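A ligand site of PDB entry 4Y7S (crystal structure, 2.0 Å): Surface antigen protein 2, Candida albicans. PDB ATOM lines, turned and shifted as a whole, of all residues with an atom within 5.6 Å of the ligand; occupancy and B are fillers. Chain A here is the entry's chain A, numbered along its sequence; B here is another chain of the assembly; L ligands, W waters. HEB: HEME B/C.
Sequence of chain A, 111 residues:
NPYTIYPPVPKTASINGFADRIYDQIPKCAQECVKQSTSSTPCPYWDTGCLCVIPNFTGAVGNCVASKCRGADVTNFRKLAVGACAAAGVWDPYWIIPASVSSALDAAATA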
ATOM      1  N   ASN A   1     -40.675   6.180  -1.356  1.00  0.00           N
ATOM      2  CA  ASN A   1     -39.309   6.621  -1.050  1.00  0.00           C
ATOM      3  C   ASN A   1     -38.295   5.771  -1.804  1.00  0.00           C
ATOM      4  O   ASN A   1     -38.513   4.577  -2.024  1.00  0.00           O
ATOM      5  CB  ASN A   1     -39.068   6.567   0.467  1.00  0.00           C
ATOM      6  CG  ASN A   1     -38.924   5.154   0.987  1.00  0.00           C
ATOM      7  OD1 ASN A   1     -37.945   4.463   0.696  1.00  0.00           O
ATOM      8  ND2 ASN A   1     -39.938   4.687   1.711  1.00  0.00           N
ATOM      9  N   TYR A   3     -35.542   4.429  -1.110  1.00  0.00           N
ATOM     10  CA  TYR A   3     -34.600   3.561  -0.396  1.00  0.00           C
ATOM     11  C   TYR A   3     -35.099   2.121  -0.228  1.00  0.00           C
ATOM     12  O   TYR A   3     -34.389   1.289   0.343  1.00  0.00           O
ATOM     13  CB  TYR A   3     -34.297   4.158   0.989  1.00  0.00           C
ATOM     14  CG  TYR A   3     -33.765   5.596   0.919  1.00  0.00           C
ATOM     15  CD1 TYR A   3     -32.477   5.869   0.487  1.00  0.00           C
ATOM     16  CD2 TYR A   3     -34.581   6.661   1.272  1.00  0.00           C
ATOM     17  CE1 TYR A   3     -32.013   7.180   0.408  1.00  0.00           C
ATOM     18  CE2 TYR A   3     -34.116   7.973   1.213  1.00  0.00           C
ATOM     19  CZ  TYR A   3     -32.837   8.218   0.772  1.00  0.00           C
ATOM     20  OH  TYR A   3     -32.393   9.534   0.694  1.00  0.00           O
ATOM     21  N   THR A   4     -36.296   1.814  -0.750  1.00  0.00           N
ATOM     22  CA  THR A   4     -36.861   0.474  -0.625  1.00  0.00           C
ATOM     23  C   THR A   4     -36.314  -0.491  -1.674  1.00  0.00           C
ATOM     24  O   THR A   4     -36.619  -1.684  -1.639  1.00  0.00           O
ATOM     25  CB  THR A   4     -38.403   0.484  -0.740  1.00  0.00           C
ATOM     26  OG1 THR A   4     -38.795   0.898  -2.072  1.00  0.00           O
ATOM     27  CG2 THR A   4     -39.020   1.418   0.313  1.00  0.00           C
ATOM     28  N   TYR A   6     -33.342  -1.057  -1.627  1.00  0.00           N
ATOM     29  CA  TYR A   6     -32.192  -1.576  -0.883  1.00  0.00           C
ATOM     30  C   TYR A   6     -32.681  -2.525   0.198  1.00  0.00           C
ATOM     31  O   TYR A   6     -33.841  -2.463   0.595  1.00  0.00           O
ATOM     32  CB  TYR A   6     -31.377  -0.442  -0.264  1.00  0.00           C
ATOM     33  CG  TYR A   6     -30.816   0.500  -1.298  1.00  0.00           C
ATOM     34  CD1 TYR A   6     -29.915   0.064  -2.263  1.00  0.00           C
ATOM     35  CD2 TYR A   6     -31.197   1.840  -1.322  1.00  0.00           C
ATOM     36  CE1 TYR A   6     -29.434   0.941  -3.228  1.00  0.00           C
ATOM     37  CE2 TYR A   6     -30.706   2.714  -2.278  1.00  0.00           C
ATOM     38  CZ  TYR A   6     -29.822   2.254  -3.221  1.00  0.00           C
ATOM     39  OH  TYR A   6     -29.341   3.130  -4.176  1.00  0.00           O
ATOM     40  N   PRO A   7     -31.806  -3.424   0.655  1.00  0.00           N
ATOM     41  CA  PRO A   7     -32.169  -4.268   1.804  1.00  0.00           C
ATOM     42  C   PRO A   7     -32.407  -3.441   3.048  1.00  0.00           C
ATOM     43  O   PRO A   7     -31.739  -2.420   3.249  1.00  0.00           O
ATOM     44  CB  PRO A   7     -30.964  -5.189   1.978  1.00  0.00           C
ATOM     45  CG  PRO A   7     -29.856  -4.541   1.250  1.00  0.00           C
ATOM     46  CD  PRO A   7     -30.468  -3.755   0.136  1.00  0.00           C
ATOM     47  N   PRO A   8     -33.381  -3.851   3.877  1.00  0.00           N
ATOM     48  CA  PRO A   8     -33.610  -3.100   5.105  1.00  0.00           C
ATOM     49  C   PRO A   8     -32.407  -3.130   6.048  1.00  0.00           C
ATOM     50  O   PRO A   8     -31.533  -4.024   5.994  1.00  0.00           O
ATOM     51  CB  PRO A   8     -34.853  -3.771   5.710  1.00  0.00           C
ATOM     52  CG  PRO A   8     -34.892  -5.139   5.112  1.00  0.00           C
ATOM     53  CD  PRO A   8     -34.291  -4.996   3.734  1.00  0.00           C
ATOM     54  N   VAL A   9     -32.320  -2.084   6.864  1.00  0.00           N
ATOM     55  CA  VAL A   9     -31.268  -1.920   7.861  1.00  0.00           C
ATOM     56  C   VAL A   9     -31.906  -1.584   9.222  1.00  0.00           C
ATOM     57  O   VAL A   9     -32.961  -0.952   9.250  1.00  0.00           O
ATOM     58  CB  VAL A   9     -30.298  -0.804   7.402  1.00  0.00           C
ATOM     59  CG1 VAL A   9     -31.027   0.533   7.243  1.00  0.00           C
ATOM     60  CG2 VAL A   9     -29.139  -0.665   8.336  1.00  0.00           C
ATOM     61  N   LYS A  11     -32.825   0.574  12.281  1.00  0.00           N
ATOM     62  CA  LYS A  11     -32.832   2.043  12.353  1.00  0.00           C
ATOM     63  C   LYS A  11     -32.298   2.580  13.692  1.00  0.00           C
ATOM     64  O   LYS A  11     -32.754   3.614  14.191  1.00  0.00           O
ATOM     65  CB  LYS A  11     -34.239   2.566  12.072  1.00  0.00           C
ATOM     66  CG  LYS A  11     -34.637   2.366  10.617  1.00  0.00           C
ATOM     67  CD  LYS A  11     -36.114   2.571  10.417  1.00  0.00           C
ATOM     68  CE  LYS A  11     -36.483   2.468   8.955  1.00  0.00           C
ATOM     69  NZ  LYS A  11     -37.923   2.733   8.730  1.00  0.00           N
ATOM     70  N   PRO A  42     -25.001  13.991   5.915  1.00  0.00           N
ATOM     71  CA  PRO A  42     -26.462  14.029   5.785  1.00  0.00           C
ATOM     72  C   PRO A  42     -27.117  12.679   6.144  1.00  0.00           C
ATOM     73  O   PRO A  42     -28.286  12.484   5.835  1.00  0.00           O
ATOM     74  CB  PRO A  42     -26.660  14.334   4.311  1.00  0.00           C
ATOM     75  CG  PRO A  42     -25.462  13.605   3.651  1.00  0.00           C
ATOM     76  CD  PRO A  42     -24.338  13.767   4.616  1.00  0.00           C
ATOM     77  N   CYS A  43     -26.356  11.771   6.738  1.00  0.00           N
ATOM     78  CA  CYS A  43     -26.823  10.400   6.971  1.00  0.00           C
ATOM     79  C   CYS A  43     -27.536  10.233   8.305  1.00  0.00           C
ATOM     80  O   CYS A  43     -27.010  10.698   9.327  1.00  0.00           O
ATOM     81  CB  CYS A  43     -25.652   9.414   6.980  1.00  0.00           C
ATOM     82  SG  CYS A  43     -24.579   9.395   5.541  1.00  0.00           S
ATOM     83  N   PRO A  44     -28.678   9.532   8.316  1.00  0.00           N
ATOM     84  CA  PRO A  44     -29.055   9.016   9.626  1.00  0.00           C
ATOM     85  C   PRO A  44     -27.916   8.194  10.178  1.00  0.00           C
ATOM     86  O   PRO A  44     -27.271   7.472   9.422  1.00  0.00           O
ATOM     87  CB  PRO A  44     -30.284   8.151   9.330  1.00  0.00           C
ATOM     88  CG  PRO A  44     -30.801   8.635   8.040  1.00  0.00           C
ATOM     89  CD  PRO A  44     -29.592   9.063   7.260  1.00  0.00           C
ATOM     90  N   TRP A  46     -27.589   5.571  11.726  1.00  0.00           N
ATOM     91  CA  TRP A  46     -27.746   4.115  11.609  1.00  0.00           C
ATOM     92  C   TRP A  46     -27.663   3.632  10.161  1.00  0.00           C
ATOM     93  O   TRP A  46     -27.722   2.451   9.903  1.00  0.00           O
ATOM     94  CB  TRP A  46     -29.099   3.674  12.205  1.00  0.00           C
ATOM     95  CG  TRP A  46     -30.240   4.515  11.763  1.00  0.00           C
ATOM     96  CD1 TRP A  46     -30.871   5.503  12.502  1.00  0.00           C
ATOM     97  CD2 TRP A  46     -30.905   4.490  10.489  1.00  0.00           C
ATOM     98  NE1 TRP A  46     -31.867   6.082  11.758  1.00  0.00           N
ATOM     99  CE2 TRP A  46     -31.919   5.476  10.524  1.00  0.00           C
ATOM    100  CE3 TRP A  46     -30.751   3.725   9.335  1.00  0.00           C
ATOM    101  CZ2 TRP A  46     -32.760   5.724   9.442  1.00  0.00           C
ATOM    102  CZ3 TRP A  46     -31.592   3.974   8.253  1.00  0.00           C
ATOM    103  CH2 TRP A  46     -32.583   4.965   8.317  1.00  0.00           C
ATOM    104  N   ASP A  47     -27.519   4.566   9.226  1.00  0.00           N
ATOM    105  CA  ASP A  47     -27.653   4.262   7.816  1.00  0.00           C
ATOM    106  C   ASP A  47     -26.332   3.811   7.165  1.00  0.00           C
ATOM    107  O   ASP A  47     -25.547   4.615   6.702  1.00  0.00           O
ATOM    108  CB  ASP A  47     -28.218   5.493   7.135  1.00  0.00           C
ATOM    109  CG  ASP A  47     -28.558   5.278   5.688  1.00  0.00           C
ATOM    110  OD1 ASP A  47     -28.174   4.255   5.061  1.00  0.00           O
ATOM    111  OD2 ASP A  47     -29.226   6.175   5.172  1.00  0.00           O
ATOM    112  N   GLY A  49     -25.561   2.241   4.278  1.00  0.00           N
ATOM    113  CA  GLY A  49     -25.364   2.647   2.891  1.00  0.00           C
ATOM    114  C   GLY A  49     -24.946   4.091   2.747  1.00  0.00           C
ATOM    115  O   GLY A  49     -24.012   4.393   2.007  1.00  0.00           O
ATOM    116  N   CYS A  50     -25.613   4.993   3.453  1.00  0.00           N
ATOM    117  CA  CYS A  50     -25.225   6.400   3.392  1.00  0.00           C
ATOM    118  C   CYS A  50     -23.778   6.603   3.909  1.00  0.00           C
ATOM    119  O   CYS A  50     -22.986   7.299   3.282  1.00  0.00           O
ATOM    120  CB  CYS A  50     -26.199   7.242   4.196  1.00  0.00           C
ATOM    121  SG  CYS A  50     -25.926   9.011   4.068  1.00  0.00           S
ATOM    122  N   VAL A  53     -20.961   5.973   1.440  1.00  0.00           N
ATOM    123  CA  VAL A  53     -20.801   6.769   0.242  1.00  0.00           C
ATOM    124  C   VAL A  53     -20.490   8.241   0.491  1.00  0.00           C
ATOM    125  O   VAL A  53     -20.282   8.967  -0.464  1.00  0.00           O
ATOM    126  CB  VAL A  53     -22.062   6.670  -0.691  1.00  0.00           C
ATOM    127  CG1 VAL A  53     -22.387   5.221  -0.961  1.00  0.00           C
ATOM    128  CG2 VAL A  53     -23.283   7.399  -0.120  1.00  0.00           C
ATOM    129  N   ILE A  54     -20.496   8.719   1.736  1.00  0.00           N
ATOM    130  CA  ILE A  54     -20.184  10.128   1.979  1.00  0.00           C
ATOM    131  C   ILE A  54     -18.674  10.249   2.198  1.00  0.00           C
ATOM    132  O   ILE A  54     -18.170   9.813   3.235  1.00  0.00           O
ATOM    133  CB  ILE A  54     -20.942  10.707   3.190  1.00  0.00           C
ATOM    134  CG1 ILE A  54     -22.459  10.561   3.023  1.00  0.00           C
ATOM    135  CG2 ILE A  54     -20.561  12.177   3.386  1.00  0.00           C
ATOM    136  CD1 ILE A  54     -23.039  11.287   1.801  1.00  0.00           C
ATOM    137  N   ALA A  88     -25.187  -3.776   1.956  1.00  0.00           N
ATOM    138  CA  ALA A  88     -26.166  -2.723   2.196  1.00  0.00           C
ATOM    139  C   ALA A  88     -26.831  -2.248   0.912  1.00  0.00           C
ATOM    140  O   ALA A  88     -27.813  -1.511   0.960  1.00  0.00           O
ATOM    141  CB  ALA A  88     -25.525  -1.553   2.900  1.00  0.00           C
ATOM    142  N   GLY A  89     -26.266  -2.641  -0.232  1.00  0.00           N
ATOM    143  CA  GLY A  89     -26.827  -2.343  -1.539  1.00  0.00           C
ATOM    144  C   GLY A  89     -26.101  -1.253  -2.307  1.00  0.00           C
ATOM    145  O   GLY A  89     -26.555  -0.822  -3.357  1.00  0.00           O
ATOM    146  N   VAL A  90     -24.951  -0.819  -1.801  1.00  0.00           N
ATOM    147  CA  VAL A  90     -24.187   0.216  -2.468  1.00  0.00           C
ATOM    148  C   VAL A  90     -23.588  -0.332  -3.754  1.00  0.00           C
ATOM    149  O   VAL A  90     -23.256  -1.510  -3.838  1.00  0.00           O
ATOM    150  CB  VAL A  90     -23.058   0.758  -1.566  1.00  0.00           C
ATOM    151  CG1 VAL A  90     -22.349   1.891  -2.246  1.00  0.00           C
ATOM    152  CG2 VAL A  90     -23.605   1.232  -0.248  1.00  0.00           C
ATOM    153  N   TRP A  91     -23.450   0.548  -4.735  1.00  0.00           N
ATOM    154  CA  TRP A  91     -22.818   0.220  -6.016  1.00  0.00           C
ATOM    155  C   TRP A  91     -21.302   0.121  -5.925  1.00  0.00           C
ATOM    156  O   TRP A  91     -20.682   0.706  -5.024  1.00  0.00           O
ATOM    157  CB  TRP A  91     -23.203   1.278  -7.066  1.00  0.00           C
ATOM    158  CG  TRP A  91     -22.857   2.673  -6.603  1.00  0.00           C
ATOM    159  CD1 TRP A  91     -21.702   3.365  -6.825  1.00  0.00           C
ATOM    160  CD2 TRP A  91     -23.690   3.535  -5.807  1.00  0.00           C
ATOM    161  NE1 TRP A  91     -21.763   4.605  -6.235  1.00  0.00           N
ATOM    162  CE2 TRP A  91     -22.972   4.729  -5.609  1.00  0.00           C
ATOM    163  CE3 TRP A  91     -24.975   3.404  -5.263  1.00  0.00           C
ATOM    164  CZ2 TRP A  91     -23.495   5.801  -4.869  1.00  0.00           C
ATOM    165  CZ3 TRP A  91     -25.499   4.475  -4.532  1.00  0.00           C
ATOM    166  CH2 TRP A  91     -24.755   5.651  -4.344  1.00  0.00           C
ATOM    167  N   VAL B  82     -29.415  14.311  -5.005  1.00  0.00           N
ATOM    168  CA  VAL B  82     -28.668  14.662  -3.805  1.00  0.00           C
ATOM    169  C   VAL B  82     -27.716  13.536  -3.437  1.00  0.00           C
ATOM    170  O   VAL B  82     -26.544  13.779  -3.171  1.00  0.00           O
ATOM    171  CB  VAL B  82     -29.617  14.949  -2.618  1.00  0.00           C
ATOM    172  CG1 VAL B  82     -28.898  14.868  -1.301  1.00  0.00           C
ATOM    173  CG2 VAL B  82     -30.272  16.326  -2.803  1.00  0.00           C
ATOM    174  N   GLY B  83     -28.209  12.310  -3.463  1.00  0.00           N
ATOM    175  CA  GLY B  83     -27.378  11.165  -3.119  1.00  0.00           C
ATOM    176  C   GLY B  83     -26.162  11.018  -4.025  1.00  0.00           C
ATOM    177  O   GLY B  83     -25.069  10.757  -3.544  1.00  0.00           O
ATOM    178  N   ALA B  86     -23.749  13.986  -3.404  1.00  0.00           N
ATOM    179  CA  ALA B  86     -23.083  13.801  -2.128  1.00  0.00           C
ATOM    180  C   ALA B  86     -21.990  12.735  -2.251  1.00  0.00           C
ATOM    181  O   ALA B  86     -20.887  12.901  -1.737  1.00  0.00           O
ATOM    182  CB  ALA B  86     -24.086  13.410  -1.029  1.00  0.00           C
ATOM    183  N   TYR B  94     -25.423  19.570  -1.732  1.00  0.00           N
ATOM    184  CA  TYR B  94     -25.033  18.445  -2.594  1.00  0.00           C
ATOM    185  C   TYR B  94     -25.510  18.615  -4.028  1.00  0.00           C
ATOM    186  O   TYR B  94     -24.690  18.791  -4.936  1.00  0.00           O
ATOM    187  CB  TYR B  94     -25.520  17.116  -1.992  1.00  0.00           C
ATOM    188  CG  TYR B  94     -25.136  17.017  -0.528  1.00  0.00           C
ATOM    189  CD1 TYR B  94     -23.816  16.902  -0.147  1.00  0.00           C
ATOM    190  CD2 TYR B  94     -26.106  17.069   0.483  1.00  0.00           C
ATOM    191  CE1 TYR B  94     -23.454  16.850   1.154  1.00  0.00           C
ATOM    192  CE2 TYR B  94     -25.764  17.022   1.785  1.00  0.00           C
ATOM    193  CZ  TYR B  94     -24.435  16.903   2.136  1.00  0.00           C
ATOM    194  OH  TYR B  94     -24.066  16.839   3.447  1.00  0.00           O
HETATM  195 FE   HEB L   1     -30.201   6.287   3.242  1.00  0.00          FE
HETATM  196  CHA HEB L   1     -33.177   5.871   4.909  1.00  0.00           C
HETATM  197  CHB HEB L   1     -30.231   2.930   2.452  1.00  0.00           C
HETATM  198  CHC HEB L   1     -27.762   6.784   0.851  1.00  0.00           C
HETATM  199  CHD HEB L   1     -30.446   9.676   3.520  1.00  0.00           C
HETATM  200  NA  HEB L   1     -31.493   4.683   3.594  1.00  0.00           N
HETATM  201  C1A HEB L   1     -32.636   4.735   4.352  1.00  0.00           C
HETATM  202  C2A HEB L   1     -33.171   3.394   4.455  1.00  0.00           C
HETATM  203  C3A HEB L   1     -32.360   2.588   3.767  1.00  0.00           C
HETATM  204  C4A HEB L   1     -31.291   3.375   3.213  1.00  0.00           C
HETATM  205  CMA HEB L   1     -32.499   1.059   3.574  1.00  0.00           C
HETATM  206  CAA HEB L   1     -34.468   3.022   5.215  1.00  0.00           C
HETATM  207  CBA HEB L   1     -35.583   2.791   4.204  1.00  0.00           C
HETATM  208  CGA HEB L   1     -36.838   2.286   4.880  1.00  0.00           C
HETATM  209  O1A HEB L   1     -37.615   1.535   4.237  1.00  0.00           O
HETATM  210  O2A HEB L   1     -37.080   2.639   6.053  1.00  0.00           O
HETATM  211  NB  HEB L   1     -29.261   5.124   1.907  1.00  0.00           N
HETATM  212  C1B HEB L   1     -29.325   3.736   1.793  1.00  0.00           C
HETATM  213  C2B HEB L   1     -28.296   3.308   0.872  1.00  0.00           C
HETATM  214  C3B HEB L   1     -27.636   4.392   0.468  1.00  0.00           C
HETATM  215  C4B HEB L   1     -28.217   5.525   1.096  1.00  0.00           C
HETATM  216  CMB HEB L   1     -28.000   1.857   0.465  1.00  0.00           C
HETATM  217  CAB HEB L   1     -26.444   4.561  -0.506  1.00  0.00           C
HETATM  218  CBB HEB L   1     -26.133   3.633  -1.406  1.00  0.00           C
HETATM  219  NC  HEB L   1     -29.303   7.911   2.313  1.00  0.00           N
HETATM  220  C1C HEB L   1     -28.246   7.896   1.437  1.00  0.00           C
HETATM  221  C2C HEB L   1     -27.742   9.248   1.233  1.00  0.00           C
HETATM  222  C3C HEB L   1     -28.501  10.046   2.000  1.00  0.00           C
HETATM  223  C4C HEB L   1     -29.488   9.211   2.674  1.00  0.00           C
HETATM  224  CMC HEB L   1     -26.542   9.586   0.319  1.00  0.00           C
HETATM  225  CAC HEB L   1     -28.448  11.568   2.197  1.00  0.00           C
HETATM  226  CBC HEB L   1     -27.711  12.342   1.417  1.00  0.00           C
HETATM  227  ND  HEB L   1     -31.620   7.569   4.038  1.00  0.00           N
HETATM  228  C1D HEB L   1     -31.447   8.944   4.108  1.00  0.00           C
HETATM  229  C2D HEB L   1     -32.462   9.498   4.961  1.00  0.00           C
HETATM  230  C3D HEB L   1     -33.329   8.309   5.390  1.00  0.00           C
HETATM  231  C4D HEB L   1     -32.721   7.159   4.772  1.00  0.00           C
HETATM  232  CMD HEB L   1     -32.656  10.979   5.331  1.00  0.00           C
HETATM  233  CAD HEB L   1     -34.539   8.330   6.323  1.00  0.00           C
HETATM  234  CBD HEB L   1     -35.853   8.533   5.596  1.00  0.00           C
HETATM  235  CGD HEB L   1     -36.908   8.862   6.634  1.00  0.00           C
HETATM  236  O1D HEB L   1     -36.615   8.793   7.859  1.00  0.00           O
HETATM  237  O2D HEB L   1     -38.051   9.194   6.212  1.00  0.00           O
HETATM  238  O   HOH W   1     -35.958  10.193   2.883  1.00  0.00           O
HETATM  239  O   HOH W   2     -28.266   1.351   4.799  1.00  0.00           O
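Water W2 bridges N of Gly 49 (2.9 Å) and OD1 of Asp 47 (2.9 Å).
Residues that only touch the ligand: Tyr 3 (3.4 Å), Tyr 6 (3.6 Å), Pro 7 (3.6 Å), Val 9 (3.99 Å), Pro 42 (3.4 Å), Pro 44 (3.6 Å), Trp 46 (3.6 Å), Gly 49 (3.5 Å), Cys 50 (3.4 Å), Val 53 (3.9 Å), Ala 88 (3.4 Å), Val 90 (3.7 Å), Trp 91 (3.3 Å), Val 82 of chain B (3.9 Å) and Gly 83 of chain B (3.9 Å).
Along chain A the residues within 4 Å of the ligand span positions 3 to 91.
OD2 of Asp 47 is bound to FE of the ligand.
NZ of Lys 11 lies within salt-bridge range of O2A of the ligand (2.8 Å).
SG of Cys 43 forms a disulfide with SG of Cys 50.
N of Tyr 3 lies within hydrogen-bond range of OD1 of Asn 1 (3.0 Å).
The backbone NH (N) of Cys 50 is in hydrogen-bond range of the side-chain carboxylate (OD1) of Asp 47, 3.1 Å away.
OD1 of Asp 47 sits close to N of Gly 49 (3.4 Å).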
